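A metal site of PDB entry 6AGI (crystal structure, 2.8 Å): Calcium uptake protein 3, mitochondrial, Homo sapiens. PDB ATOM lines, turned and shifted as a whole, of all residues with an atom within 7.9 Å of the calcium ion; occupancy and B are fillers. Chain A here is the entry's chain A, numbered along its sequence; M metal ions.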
ATOM      1  N   SER A 322      15.307 -26.481  21.207  1.00  0.00           N
ATOM      2  CA  SER A 322      15.267 -25.313  22.074  1.00  0.00           C
ATOM      3  C   SER A 322      15.864 -24.107  21.352  1.00  0.00           C
ATOM      4  O   SER A 322      16.842 -24.254  20.598  1.00  0.00           O
ATOM      5  CB  SER A 322      16.045 -25.556  23.366  1.00  0.00           C
ATOM      6  OG  SER A 322      15.407 -26.518  24.167  1.00  0.00           O
ATOM      7  N   ILE A 323      15.238 -22.883  21.572  1.00  0.00           N
ATOM      8  CA  ILE A 323      15.773 -21.655  21.000  1.00  0.00           C
ATOM      9  C   ILE A 323      16.743 -21.005  21.985  1.00  0.00           C
ATOM     10  O   ILE A 323      16.595 -21.084  23.209  1.00  0.00           O
ATOM     11  CB  ILE A 323      14.661 -20.665  20.560  1.00  0.00           C
ATOM     12  CG1 ILE A 323      13.515 -20.515  21.568  1.00  0.00           C
ATOM     13  CG2 ILE A 323      14.034 -21.096  19.317  1.00  0.00           C
ATOM     14  CD1 ILE A 323      13.849 -19.694  22.772  1.00  0.00           C
ATOM     15  N   PHE A 349      14.665 -15.361  29.907  1.00  0.00           N
ATOM     16  CA  PHE A 349      15.454 -16.570  29.946  1.00  0.00           C
ATOM     17  C   PHE A 349      15.825 -16.943  31.376  1.00  0.00           C
ATOM     18  O   PHE A 349      15.725 -18.108  31.780  1.00  0.00           O
ATOM     19  CB  PHE A 349      16.709 -16.424  29.080  1.00  0.00           C
ATOM     20  CG  PHE A 349      16.519 -16.898  27.683  1.00  0.00           C
ATOM     21  CD1 PHE A 349      15.458 -16.407  26.925  1.00  0.00           C
ATOM     22  CD2 PHE A 349      17.324 -17.910  27.148  1.00  0.00           C
ATOM     23  CE1 PHE A 349      15.240 -16.847  25.629  1.00  0.00           C
ATOM     24  CE2 PHE A 349      17.112 -18.378  25.849  1.00  0.00           C
ATOM     25  CZ  PHE A 349      16.066 -17.846  25.090  1.00  0.00           C
ATOM     26  N   PHE A 352      12.655 -18.264  33.119  1.00  0.00           N
ATOM     27  CA  PHE A 352      12.128 -19.524  32.608  1.00  0.00           C
ATOM     28  C   PHE A 352      13.187 -20.547  32.178  1.00  0.00           C
ATOM     29  O   PHE A 352      12.859 -21.741  32.146  1.00  0.00           O
ATOM     30  CB  PHE A 352      11.197 -19.274  31.424  1.00  0.00           C
ATOM     31  CG  PHE A 352       9.950 -18.482  31.746  1.00  0.00           C
ATOM     32  CD1 PHE A 352       8.864 -19.101  32.360  1.00  0.00           C
ATOM     33  CD2 PHE A 352       9.843 -17.147  31.397  1.00  0.00           C
ATOM     34  CE1 PHE A 352       7.714 -18.390  32.646  1.00  0.00           C
ATOM     35  CE2 PHE A 352       8.691 -16.435  31.668  1.00  0.00           C
ATOM     36  CZ  PHE A 352       7.629 -17.042  32.293  1.00  0.00           C
ATOM     37  N   ASP A 353      14.429 -20.164  31.874  1.00  0.00           N
ATOM     38  CA  ASP A 353      15.340 -21.211  31.382  1.00  0.00           C
ATOM     39  C   ASP A 353      15.843 -21.934  32.624  1.00  0.00           C
ATOM     40  O   ASP A 353      16.844 -21.579  33.233  1.00  0.00           O
ATOM     41  CB  ASP A 353      16.504 -20.679  30.576  1.00  0.00           C
ATOM     42  CG  ASP A 353      17.635 -21.675  30.515  1.00  0.00           C
ATOM     43  OD1 ASP A 353      17.321 -22.897  30.465  1.00  0.00           O
ATOM     44  OD2 ASP A 353      18.805 -21.256  30.630  1.00  0.00           O
ATOM     45  N   VAL A 354      15.175 -23.022  32.898  1.00  0.00           N
ATOM     46  CA  VAL A 354      15.334 -23.679  34.177  1.00  0.00           C
ATOM     47  C   VAL A 354      16.358 -24.805  34.113  1.00  0.00           C
ATOM     48  O   VAL A 354      17.109 -25.004  35.067  1.00  0.00           O
ATOM     49  CB  VAL A 354      13.930 -24.162  34.604  1.00  0.00           C
ATOM     50  CG1 VAL A 354      14.087 -25.294  35.432  1.00  0.00           C
ATOM     51  CG2 VAL A 354      13.149 -23.046  35.314  1.00  0.00           C
ATOM     52  N   ASP A 355      16.385 -25.549  32.986  1.00  0.00           N
ATOM     53  CA  ASP A 355      17.519 -26.382  32.581  1.00  0.00           C
ATOM     54  C   ASP A 355      18.872 -25.709  32.756  1.00  0.00           C
ATOM     55  O   ASP A 355      19.892 -26.399  32.863  1.00  0.00           O
ATOM     56  CB  ASP A 355      17.362 -26.829  31.122  1.00  0.00           C
ATOM     57  CG  ASP A 355      16.066 -27.606  30.873  1.00  0.00           C
ATOM     58  OD1 ASP A 355      15.218 -27.679  31.792  1.00  0.00           O
ATOM     59  OD2 ASP A 355      15.892 -28.120  29.744  1.00  0.00           O
ATOM     60  N   LYS A 356      18.921 -24.374  32.695  1.00  0.00           N
ATOM     61  CA  LYS A 356      20.172 -23.634  32.728  1.00  0.00           C
ATOM     62  C   LYS A 356      21.087 -24.072  31.579  1.00  0.00           C
ATOM     63  O   LYS A 356      22.283 -24.323  31.773  1.00  0.00           O
ATOM     64  CB  LYS A 356      20.868 -23.792  34.075  1.00  0.00           C
ATOM     65  CG  LYS A 356      19.963 -23.556  35.282  1.00  0.00           C
ATOM     66  CD  LYS A 356      19.864 -22.078  35.659  1.00  0.00           C
ATOM     67  CE  LYS A 356      19.018 -21.850  36.912  1.00  0.00           C
ATOM     68  NZ  LYS A 356      19.637 -20.852  37.844  1.00  0.00           N
ATOM     69  N   ASP A 357      20.504 -24.175  30.383  1.00  0.00           N
ATOM     70  CA  ASP A 357      21.244 -24.377  29.151  1.00  0.00           C
ATOM     71  C   ASP A 357      21.383 -23.080  28.337  1.00  0.00           C
ATOM     72  O   ASP A 357      21.941 -23.117  27.240  1.00  0.00           O
ATOM     73  CB  ASP A 357      20.592 -25.468  28.313  1.00  0.00           C
ATOM     74  CG  ASP A 357      19.149 -25.155  27.966  1.00  0.00           C
ATOM     75  OD1 ASP A 357      18.677 -24.061  28.317  1.00  0.00           O
ATOM     76  OD2 ASP A 357      18.491 -26.004  27.338  1.00  0.00           O
ATOM     77  N   ASP A 358      20.828 -21.968  28.833  1.00  0.00           N
ATOM     78  CA  ASP A 358      20.657 -20.724  28.087  1.00  0.00           C
ATOM     79  C   ASP A 358      19.897 -20.959  26.786  1.00  0.00           C
ATOM     80  O   ASP A 358      20.149 -20.337  25.754  1.00  0.00           O
ATOM     81  CB  ASP A 358      21.999 -20.013  27.856  1.00  0.00           C
ATOM     82  CG  ASP A 358      21.869 -18.475  27.868  1.00  0.00           C
ATOM     83  OD1 ASP A 358      20.887 -17.950  28.444  1.00  0.00           O
ATOM     84  OD2 ASP A 358      22.755 -17.792  27.294  1.00  0.00           O
ATOM     85  N   GLN A 359      18.926 -21.863  26.866  1.00  0.00           N
ATOM     86  CA  GLN A 359      17.975 -22.099  25.801  1.00  0.00           C
ATOM     87  C   GLN A 359      16.618 -22.374  26.412  1.00  0.00           C
ATOM     88  O   GLN A 359      16.514 -22.832  27.541  1.00  0.00           O
ATOM     89  CB  GLN A 359      18.380 -23.273  24.918  1.00  0.00           C
ATOM     90  CG  GLN A 359      19.588 -22.994  24.053  1.00  0.00           C
ATOM     91  CD  GLN A 359      19.667 -23.971  22.903  1.00  0.00           C
ATOM     92  OE1 GLN A 359      18.909 -24.951  22.853  1.00  0.00           O
ATOM     93  NE2 GLN A 359      20.570 -23.718  21.955  1.00  0.00           N
ATOM     94  N   LEU A 360      15.580 -22.162  25.612  1.00  0.00           N
ATOM     95  CA  LEU A 360      14.213 -22.358  26.071  1.00  0.00           C
ATOM     96  C   LEU A 360      13.590 -23.452  25.228  1.00  0.00           C
ATOM     97  O   LEU A 360      13.614 -23.374  23.997  1.00  0.00           O
ATOM     98  CB  LEU A 360      13.374 -21.083  25.944  1.00  0.00           C
ATOM     99  CG  LEU A 360      13.290 -20.106  27.124  1.00  0.00           C
ATOM    100  CD1 LEU A 360      12.417 -20.654  28.237  1.00  0.00           C
ATOM    101  CD2 LEU A 360      14.637 -19.731  27.658  1.00  0.00           C
ATOM    102  N   SER A 361      13.106 -24.477  25.904  1.00  0.00           N
ATOM    103  CA  SER A 361      12.410 -25.585  25.275  1.00  0.00           C
ATOM    104  C   SER A 361      10.915 -25.317  25.331  1.00  0.00           C
ATOM    105  O   SER A 361      10.438 -24.464  26.071  1.00  0.00           O
ATOM    106  CB  SER A 361      12.721 -26.893  25.985  1.00  0.00           C
ATOM    107  OG  SER A 361      11.872 -27.030  27.102  1.00  0.00           O
ATOM    108  N   TYR A 362      10.155 -26.106  24.566  1.00  0.00           N
ATOM    109  CA  TYR A 362       8.727 -25.868  24.449  1.00  0.00           C
ATOM    110  C   TYR A 362       8.066 -25.923  25.811  1.00  0.00           C
ATOM    111  O   TYR A 362       7.137 -25.158  26.096  1.00  0.00           O
ATOM    112  CB  TYR A 362       8.065 -26.876  23.510  1.00  0.00           C
ATOM    113  CG  TYR A 362       6.560 -26.858  23.604  1.00  0.00           C
ATOM    114  CD1 TYR A 362       5.883 -27.608  24.568  1.00  0.00           C
ATOM    115  CD2 TYR A 362       5.801 -26.056  22.752  1.00  0.00           C
ATOM    116  CE1 TYR A 362       4.509 -27.570  24.690  1.00  0.00           C
ATOM    117  CE2 TYR A 362       4.402 -26.022  22.856  1.00  0.00           C
ATOM    118  CZ  TYR A 362       3.767 -26.784  23.833  1.00  0.00           C
ATOM    119  OH  TYR A 362       2.402 -26.784  23.972  1.00  0.00           O
ATOM    120  N   GLU A 364       9.267 -25.271  28.741  1.00  0.00           N
ATOM    121  CA  GLU A 364       9.712 -24.216  29.643  1.00  0.00           C
ATOM    122  C   GLU A 364       8.932 -22.911  29.486  1.00  0.00           C
ATOM    123  O   GLU A 364       8.733 -22.177  30.464  1.00  0.00           O
ATOM    124  CB  GLU A 364      11.180 -23.918  29.394  1.00  0.00           C
ATOM    125  CG  GLU A 364      12.034 -25.103  29.545  1.00  0.00           C
ATOM    126  CD  GLU A 364      13.333 -24.747  30.166  1.00  0.00           C
ATOM    127  OE1 GLU A 364      14.114 -24.104  29.435  1.00  0.00           O
ATOM    128  OE2 GLU A 364      13.618 -25.150  31.314  1.00  0.00           O
HETATM  129 CA    CA M   1      16.261 -24.879  29.160  1.00  0.00          CA
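Residues that only touch the calcium ion: Asp 355.
N of Asp 355 lies within hydrogen-bond range of OE2 of Glu 364. The side-chain amide oxygen (OE1) of Gln 359 lies close to the backbone carbonyl oxygen (O) of Ser 322. The side-chain carboxylate (OD2) of Asp 353 lies within hydrogen-bond range of the backbone NH (N) of Asp 358 (2.8 Å). The side-chain carboxylate (OD1) of Asp 353 sits close to the backbone NH (N) of Lys 356 (3.1 Å). OE2 of Glu 364 sits at hydrogen-bond distance from N of Val 354 (3.1 Å).
The calcium ion is bound by the side-chain carboxylate (OE1) of Glu 364 (2.3 Å), the side-chain carboxylate (OD1) of Asp 353 (2.6 Å), the backbone carbonyl oxygen (O) of Gln 359 (2.6 Å) and the side-chain carboxylate (OD1) of Asp 357 (2.7 Å). The calcium ion has four donor atoms within binding distance. Slightly farther from the calcium ion lies the side-chain carboxylate (OD2) of Asp 357 (3.1 Å).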
